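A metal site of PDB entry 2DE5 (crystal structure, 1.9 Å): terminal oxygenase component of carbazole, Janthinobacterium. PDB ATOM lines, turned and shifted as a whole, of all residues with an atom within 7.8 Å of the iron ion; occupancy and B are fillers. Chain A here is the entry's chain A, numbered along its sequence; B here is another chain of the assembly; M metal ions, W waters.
OD1 of Asp 333 sits close to ND2 of Asn 177 (3.0 Å). The side-chain amide nitrogen (ND2) of Asn 330 is in hydrogen-bond range of the side-chain carboxylate (OD2) of Asp 333, 2.9 Å away. The backbone carbonyl oxygen of Phe 329 sits close to a ring nitrogen (ND1) of His 187 (3.3 Å). O of Asn 177 is in hydrogen-bond range of ND1 of His 183 (3.1 Å). A ring nitrogen (ND1) of His 183 is in hydrogen-bond range of the backbone carbonyl oxygen (O) of Asp 180, at 2.5 Å.
Of the 23 residues printed, 3 come within 4 Å of the iron ion.
Water W1 binds the iron ion, 1.9 Å away. OD1 of Asp 333 is bound to the iron ion (2.0 Å). A ring nitrogen (NE2) of His 187 binds the iron ion, 2.1 Å away. The iron ion is bound by NE2 of His 183 (2.1 Å). Slightly farther from the iron ion lies OD2 of Asp 333 (2.7 Å).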
ATOM      1  N   ASN A 177     -21.552  -2.682 -12.381  1.00  0.00           N
ATOM      2  CA  ASN A 177     -20.945  -1.829 -11.370  1.00  0.00           C
ATOM      3  C   ASN A 177     -21.401  -2.273  -9.985  1.00  0.00           C
ATOM      4  O   ASN A 177     -20.606  -2.349  -9.054  1.00  0.00           O
ATOM      5  CB  ASN A 177     -21.322  -0.371 -11.573  1.00  0.00           C
ATOM      6  CG  ASN A 177     -20.858   0.495 -10.409  1.00  0.00           C
ATOM      7  OD1 ASN A 177     -19.657   0.738 -10.242  1.00  0.00           O
ATOM      8  ND2 ASN A 177     -21.788   0.923  -9.587  1.00  0.00           N
ATOM      9  N   GLY A 178     -22.694  -2.565  -9.854  1.00  0.00           N
ATOM     10  CA  GLY A 178     -23.220  -2.968  -8.566  1.00  0.00           C
ATOM     11  C   GLY A 178     -22.641  -4.255  -8.015  1.00  0.00           C
ATOM     12  O   GLY A 178     -22.380  -4.363  -6.812  1.00  0.00           O
ATOM     13  N   PHE A 179     -22.420  -5.231  -8.883  1.00  0.00           N
ATOM     14  CA  PHE A 179     -21.887  -6.531  -8.504  1.00  0.00           C
ATOM     15  C   PHE A 179     -20.349  -6.606  -8.522  1.00  0.00           C
ATOM     16  O   PHE A 179     -19.754  -7.616  -8.136  1.00  0.00           O
ATOM     17  CB  PHE A 179     -22.481  -7.588  -9.442  1.00  0.00           C
ATOM     18  CG  PHE A 179     -22.301  -9.001  -8.973  1.00  0.00           C
ATOM     19  CD1 PHE A 179     -22.704  -9.386  -7.699  1.00  0.00           C
ATOM     20  CD2 PHE A 179     -21.717  -9.950  -9.804  1.00  0.00           C
ATOM     21  CE1 PHE A 179     -22.554 -10.689  -7.262  1.00  0.00           C
ATOM     22  CE2 PHE A 179     -21.547 -11.263  -9.372  1.00  0.00           C
ATOM     23  CZ  PHE A 179     -21.969 -11.639  -8.093  1.00  0.00           C
ATOM     24  N   ASP A 180     -19.717  -5.523  -8.945  1.00  0.00           N
ATOM     25  CA  ASP A 180     -18.256  -5.421  -9.052  1.00  0.00           C
ATOM     26  C   ASP A 180     -17.599  -5.369  -7.667  1.00  0.00           C
ATOM     27  O   ASP A 180     -17.685  -4.351  -6.975  1.00  0.00           O
ATOM     28  CB  ASP A 180     -17.924  -4.138  -9.818  1.00  0.00           C
ATOM     29  CG  ASP A 180     -16.467  -4.045 -10.217  1.00  0.00           C
ATOM     30  OD1 ASP A 180     -15.600  -4.582  -9.493  1.00  0.00           O
ATOM     31  OD2 ASP A 180     -16.196  -3.409 -11.261  1.00  0.00           O
ATOM     32  N   HIS A 183     -15.251  -2.277  -7.039  1.00  0.00           N
ATOM     33  CA  HIS A 183     -15.752  -0.928  -7.231  1.00  0.00           C
ATOM     34  C   HIS A 183     -15.946  -0.186  -5.916  1.00  0.00           C
ATOM     35  O   HIS A 183     -16.157   1.020  -5.915  1.00  0.00           O
ATOM     36  CB  HIS A 183     -17.054  -0.923  -8.036  1.00  0.00           C
ATOM     37  CG  HIS A 183     -18.291  -0.989  -7.194  1.00  0.00           C
ATOM     38  ND1 HIS A 183     -18.716  -2.142  -6.587  1.00  0.00           N
ATOM     39  CD2 HIS A 183     -19.193  -0.030  -6.872  1.00  0.00           C
ATOM     40  CE1 HIS A 183     -19.833  -1.904  -5.918  1.00  0.00           C
ATOM     41  NE2 HIS A 183     -20.147  -0.625  -6.085  1.00  0.00           N
ATOM     42  N   ILE A 184     -15.882  -0.910  -4.800  1.00  0.00           N
ATOM     43  CA  ILE A 184     -15.952  -0.366  -3.450  1.00  0.00           C
ATOM     44  C   ILE A 184     -15.051   0.853  -3.297  1.00  0.00           C
ATOM     45  O   ILE A 184     -15.228   1.680  -2.401  1.00  0.00           O
ATOM     46  CB  ILE A 184     -15.512  -1.462  -2.476  1.00  0.00           C
ATOM     47  CG1 ILE A 184     -15.909  -1.085  -1.048  1.00  0.00           C
ATOM     48  CG2 ILE A 184     -13.984  -1.626  -2.515  1.00  0.00           C
ATOM     49  CD1 ILE A 184     -15.822  -2.266  -0.081  1.00  0.00           C
ATOM     50  N   TYR A 185     -13.999   0.865  -4.114  1.00  0.00           N
ATOM     51  CA  TYR A 185     -12.992   1.909  -4.043  1.00  0.00           C
ATOM     52  C   TYR A 185     -13.610   3.291  -4.236  1.00  0.00           C
ATOM     53  O   TYR A 185     -13.184   4.260  -3.597  1.00  0.00           O
ATOM     54  CB  TYR A 185     -11.927   1.675  -5.123  1.00  0.00           C
ATOM     55  CG  TYR A 185     -10.783   2.669  -5.102  1.00  0.00           C
ATOM     56  CD1 TYR A 185      -9.819   2.648  -4.098  1.00  0.00           C
ATOM     57  CD2 TYR A 185     -10.660   3.647  -6.095  1.00  0.00           C
ATOM     58  CE1 TYR A 185      -8.772   3.570  -4.075  1.00  0.00           C
ATOM     59  CE2 TYR A 185      -9.628   4.576  -6.079  1.00  0.00           C
ATOM     60  CZ  TYR A 185      -8.673   4.528  -5.063  1.00  0.00           C
ATOM     61  OH  TYR A 185      -7.643   5.440  -5.043  1.00  0.00           O
ATOM     62  N   ILE A 186     -14.615   3.393  -5.101  1.00  0.00           N
ATOM     63  CA  ILE A 186     -15.257   4.681  -5.359  1.00  0.00           C
ATOM     64  C   ILE A 186     -16.070   5.181  -4.166  1.00  0.00           C
ATOM     65  O   ILE A 186     -16.520   6.327  -4.159  1.00  0.00           O
ATOM     66  CB  ILE A 186     -16.210   4.633  -6.582  1.00  0.00           C
ATOM     67  CG1 ILE A 186     -17.470   3.847  -6.240  1.00  0.00           C
ATOM     68  CG2 ILE A 186     -15.480   4.041  -7.793  1.00  0.00           C
ATOM     69  CD1 ILE A 186     -18.512   3.800  -7.371  1.00  0.00           C
ATOM     70  N   HIS A 187     -16.260   4.326  -3.176  1.00  0.00           N
ATOM     71  CA  HIS A 187     -17.030   4.691  -1.994  1.00  0.00           C
ATOM     72  C   HIS A 187     -16.175   5.038  -0.781  1.00  0.00           C
ATOM     73  O   HIS A 187     -16.713   5.319   0.290  1.00  0.00           O
ATOM     74  CB  HIS A 187     -17.951   3.540  -1.597  1.00  0.00           C
ATOM     75  CG  HIS A 187     -19.012   3.233  -2.609  1.00  0.00           C
ATOM     76  ND1 HIS A 187     -19.978   4.157  -2.969  1.00  0.00           N
ATOM     77  CD2 HIS A 187     -19.269   2.118  -3.325  1.00  0.00           C
ATOM     78  CE1 HIS A 187     -20.774   3.618  -3.872  1.00  0.00           C
ATOM     79  NE2 HIS A 187     -20.360   2.387  -4.111  1.00  0.00           N
ATOM     80  N   LEU A 270     -29.792  -6.549  -7.639  1.00  0.00           N
ATOM     81  CA  LEU A 270     -28.726  -6.810  -6.666  1.00  0.00           C
ATOM     82  C   LEU A 270     -29.268  -6.839  -5.239  1.00  0.00           C
ATOM     83  O   LEU A 270     -30.158  -6.050  -4.896  1.00  0.00           O
ATOM     84  CB  LEU A 270     -27.667  -5.708  -6.770  1.00  0.00           C
ATOM     85  CG  LEU A 270     -26.375  -5.833  -5.945  1.00  0.00           C
ATOM     86  CD1 LEU A 270     -25.423  -6.807  -6.639  1.00  0.00           C
ATOM     87  CD2 LEU A 270     -25.701  -4.476  -5.831  1.00  0.00           C
ATOM     88  N   PHE A 275     -27.053  -4.127   4.716  1.00  0.00           N
ATOM     89  CA  PHE A 275     -26.684  -2.796   4.243  1.00  0.00           C
ATOM     90  C   PHE A 275     -27.920  -1.898   4.287  1.00  0.00           C
ATOM     91  O   PHE A 275     -29.025  -2.353   4.015  1.00  0.00           O
ATOM     92  CB  PHE A 275     -26.168  -2.871   2.800  1.00  0.00           C
ATOM     93  CG  PHE A 275     -25.371  -1.673   2.387  1.00  0.00           C
ATOM     94  CD1 PHE A 275     -24.060  -1.505   2.828  1.00  0.00           C
ATOM     95  CD2 PHE A 275     -25.933  -0.693   1.571  1.00  0.00           C
ATOM     96  CE1 PHE A 275     -23.320  -0.382   2.466  1.00  0.00           C
ATOM     97  CE2 PHE A 275     -25.193   0.430   1.209  1.00  0.00           C
ATOM     98  CZ  PHE A 275     -23.898   0.588   1.647  1.00  0.00           C
ATOM     99  N   GLU A 284     -31.755  -3.641  -5.217  1.00  0.00           N
ATOM    100  CA  GLU A 284     -31.883  -2.619  -6.251  1.00  0.00           C
ATOM    101  C   GLU A 284     -31.912  -3.201  -7.650  1.00  0.00           C
ATOM    102  O   GLU A 284     -31.093  -4.059  -8.015  1.00  0.00           O
ATOM    103  CB  GLU A 284     -30.767  -1.573  -6.123  1.00  0.00           C
ATOM    104  CG  GLU A 284     -29.340  -2.085  -6.070  1.00  0.00           C
ATOM    105  CD  GLU A 284     -28.337  -0.946  -5.922  1.00  0.00           C
ATOM    106  OE1 GLU A 284     -28.643   0.009  -5.183  1.00  0.00           O
ATOM    107  OE2 GLU A 284     -27.248  -1.011  -6.524  1.00  0.00           O
ATOM    108  N   TYR A 286     -32.036  -2.604 -11.920  1.00  0.00           N
ATOM    109  CA  TYR A 286     -31.477  -1.743 -12.965  1.00  0.00           C
ATOM    110  C   TYR A 286     -32.365  -2.139 -14.151  1.00  0.00           C
ATOM    111  O   TYR A 286     -32.041  -3.060 -14.910  1.00  0.00           O
ATOM    112  CB  TYR A 286     -30.009  -2.111 -13.215  1.00  0.00           C
ATOM    113  CG  TYR A 286     -29.209  -2.247 -11.942  1.00  0.00           C
ATOM    114  CD1 TYR A 286     -28.784  -1.133 -11.217  1.00  0.00           C
ATOM    115  CD2 TYR A 286     -28.873  -3.516 -11.452  1.00  0.00           C
ATOM    116  CE1 TYR A 286     -28.048  -1.280 -10.030  1.00  0.00           C
ATOM    117  CE2 TYR A 286     -28.138  -3.659 -10.274  1.00  0.00           C
ATOM    118  CZ  TYR A 286     -27.731  -2.549  -9.571  1.00  0.00           C
ATOM    119  OH  TYR A 286     -26.995  -2.722  -8.415  1.00  0.00           O
ATOM    120  N   TYR A 296     -33.235   3.166 -11.900  1.00  0.00           N
ATOM    121  CA  TYR A 296     -32.387   2.708 -10.804  1.00  0.00           C
ATOM    122  C   TYR A 296     -33.405   2.650  -9.665  1.00  0.00           C
ATOM    123  O   TYR A 296     -33.647   3.629  -8.964  1.00  0.00           O
ATOM    124  CB  TYR A 296     -31.277   3.722 -10.517  1.00  0.00           C
ATOM    125  CG  TYR A 296     -30.394   3.373  -9.340  1.00  0.00           C
ATOM    126  CD1 TYR A 296     -30.151   2.041  -8.984  1.00  0.00           C
ATOM    127  CD2 TYR A 296     -29.776   4.372  -8.596  1.00  0.00           C
ATOM    128  CE1 TYR A 296     -29.327   1.715  -7.902  1.00  0.00           C
ATOM    129  CE2 TYR A 296     -28.950   4.058  -7.509  1.00  0.00           C
ATOM    130  CZ  TYR A 296     -28.735   2.738  -7.169  1.00  0.00           C
ATOM    131  OH  TYR A 296     -27.943   2.440  -6.084  1.00  0.00           O
ATOM    132  N   PHE A 329     -24.447   7.435  -0.513  1.00  0.00           N
ATOM    133  CA  PHE A 329     -23.541   6.347  -0.862  1.00  0.00           C
ATOM    134  C   PHE A 329     -23.659   5.995  -2.341  1.00  0.00           C
ATOM    135  O   PHE A 329     -22.679   6.039  -3.077  1.00  0.00           O
ATOM    136  CB  PHE A 329     -23.869   5.111  -0.014  1.00  0.00           C
ATOM    137  CG  PHE A 329     -22.874   3.999  -0.154  1.00  0.00           C
ATOM    138  CD1 PHE A 329     -21.702   4.004   0.589  1.00  0.00           C
ATOM    139  CD2 PHE A 329     -23.121   2.923  -1.005  1.00  0.00           C
ATOM    140  CE1 PHE A 329     -20.784   2.959   0.501  1.00  0.00           C
ATOM    141  CE2 PHE A 329     -22.212   1.876  -1.104  1.00  0.00           C
ATOM    142  CZ  PHE A 329     -21.045   1.888  -0.358  1.00  0.00           C
ATOM    143  N   ASN A 330     -24.871   5.673  -2.771  1.00  0.00           N
ATOM    144  CA  ASN A 330     -25.116   5.267  -4.155  1.00  0.00           C
ATOM    145  C   ASN A 330     -24.951   6.320  -5.251  1.00  0.00           C
ATOM    146  O   ASN A 330     -24.865   5.966  -6.435  1.00  0.00           O
ATOM    147  CB  ASN A 330     -26.486   4.603  -4.262  1.00  0.00           C
ATOM    148  CG  ASN A 330     -26.542   3.263  -3.537  1.00  0.00           C
ATOM    149  OD1 ASN A 330     -27.506   2.976  -2.817  1.00  0.00           O
ATOM    150  ND2 ASN A 330     -25.523   2.440  -3.731  1.00  0.00           N
ATOM    151  N   ASN A 331     -24.909   7.600  -4.898  1.00  0.00           N
ATOM    152  CA  ASN A 331     -24.737   8.607  -5.937  1.00  0.00           C
ATOM    153  C   ASN A 331     -23.443   8.388  -6.717  1.00  0.00           C
ATOM    154  O   ASN A 331     -23.400   8.605  -7.933  1.00  0.00           O
ATOM    155  CB  ASN A 331     -24.751  10.021  -5.348  1.00  0.00           C
ATOM    156  CG  ASN A 331     -26.156  10.595  -5.261  1.00  0.00           C
ATOM    157  OD1 ASN A 331     -27.123   9.980  -5.721  1.00  0.00           O
ATOM    158  ND2 ASN A 331     -26.279  11.790  -4.682  1.00  0.00           N
ATOM    159  N   ASP A 332     -22.387   7.942  -6.037  1.00  0.00           N
ATOM    160  CA  ASP A 332     -21.132   7.685  -6.732  1.00  0.00           C
ATOM    161  C   ASP A 332     -21.273   6.542  -7.734  1.00  0.00           C
ATOM    162  O   ASP A 332     -20.556   6.506  -8.738  1.00  0.00           O
ATOM    163  CB  ASP A 332     -20.019   7.383  -5.736  1.00  0.00           C
ATOM    164  CG  ASP A 332     -19.571   8.619  -4.978  1.00  0.00           C
ATOM    165  OD1 ASP A 332     -19.310   9.646  -5.631  1.00  0.00           O
ATOM    166  OD2 ASP A 332     -19.484   8.563  -3.733  1.00  0.00           O
ATOM    167  N   ASP A 333     -22.189   5.622  -7.476  1.00  0.00           N
ATOM    168  CA  ASP A 333     -22.395   4.506  -8.410  1.00  0.00           C
ATOM    169  C   ASP A 333     -22.982   5.044  -9.708  1.00  0.00           C
ATOM    170  O   ASP A 333     -22.642   4.572 -10.794  1.00  0.00           O
ATOM    171  CB  ASP A 333     -23.346   3.461  -7.822  1.00  0.00           C
ATOM    172  CG  ASP A 333     -22.737   2.724  -6.663  1.00  0.00           C
ATOM    173  OD1 ASP A 333     -21.638   2.162  -6.841  1.00  0.00           O
ATOM    174  OD2 ASP A 333     -23.352   2.693  -5.573  1.00  0.00           O
ATOM    175  N   ILE A 334     -23.851   6.041  -9.577  1.00  0.00           N
ATOM    176  CA  ILE A 334     -24.482   6.647 -10.741  1.00  0.00           C
ATOM    177  C   ILE A 334     -23.464   7.248 -11.711  1.00  0.00           C
ATOM    178  O   ILE A 334     -23.482   6.925 -12.899  1.00  0.00           O
ATOM    179  CB  ILE A 334     -25.508   7.731 -10.311  1.00  0.00           C
ATOM    180  CG1 ILE A 334     -26.670   7.061  -9.580  1.00  0.00           C
ATOM    181  CG2 ILE A 334     -26.022   8.487 -11.534  1.00  0.00           C
ATOM    182  CD1 ILE A 334     -27.709   8.036  -9.008  1.00  0.00           C
ATOM    183  N   ALA A 336     -20.326   6.596 -11.873  1.00  0.00           N
ATOM    184  CA  ALA A 336     -19.380   5.562 -12.311  1.00  0.00           C
ATOM    185  C   ALA A 336     -20.000   4.835 -13.520  1.00  0.00           C
ATOM    186  O   ALA A 336     -19.312   4.561 -14.503  1.00  0.00           O
ATOM    187  CB  ALA A 336     -19.119   4.569 -11.180  1.00  0.00           C
ATOM    188  N   ARG A 337     -21.293   4.540 -13.443  1.00  0.00           N
ATOM    189  CA  ARG A 337     -21.992   3.871 -14.551  1.00  0.00           C
ATOM    190  C   ARG A 337     -21.926   4.743 -15.793  1.00  0.00           C
ATOM    191  O   ARG A 337     -21.692   4.251 -16.889  1.00  0.00           O
ATOM    192  CB  ARG A 337     -23.475   3.695 -14.245  1.00  0.00           C
ATOM    193  CG  ARG A 337     -23.782   2.855 -13.060  1.00  0.00           C
ATOM    194  CD  ARG A 337     -25.265   2.891 -12.794  1.00  0.00           C
ATOM    195  NE  ARG A 337     -25.503   2.536 -11.402  1.00  0.00           N
ATOM    196  CZ  ARG A 337     -26.679   2.642 -10.800  1.00  0.00           C
ATOM    197  NH1 ARG A 337     -27.734   3.080 -11.461  1.00  0.00           N
ATOM    198  NH2 ARG A 337     -26.785   2.299  -9.519  1.00  0.00           N
ATOM    199  N   TYR B  92     -11.776   4.566 -10.454  1.00  0.00           N
ATOM    200  CA  TYR B  92     -12.720   3.445 -10.386  1.00  0.00           C
ATOM    201  C   TYR B  92     -12.248   2.236  -9.584  1.00  0.00           C
ATOM    202  O   TYR B  92     -12.830   1.909  -8.543  1.00  0.00           O
ATOM    203  CB  TYR B  92     -13.089   3.019 -11.811  1.00  0.00           C
ATOM    204  CG  TYR B  92     -14.475   2.428 -11.966  1.00  0.00           C
ATOM    205  CD1 TYR B  92     -15.247   2.078 -10.855  1.00  0.00           C
ATOM    206  CD2 TYR B  92     -15.003   2.186 -13.236  1.00  0.00           C
ATOM    207  CE1 TYR B  92     -16.515   1.491 -11.005  1.00  0.00           C
ATOM    208  CE2 TYR B  92     -16.251   1.610 -13.405  1.00  0.00           C
ATOM    209  CZ  TYR B  92     -17.001   1.263 -12.295  1.00  0.00           C
ATOM    210  OH  TYR B  92     -18.244   0.683 -12.477  1.00  0.00           O
HETATM  211 FE    FE M   1     -21.394   0.907  -5.239  1.00  0.00          FE
HETATM  212  O   HOH W   1     -22.945   0.016  -4.563  1.00  0.00           O
HETATM  213  O   HOH W   2     -21.364  -1.096  -2.851  1.00  0.00           O
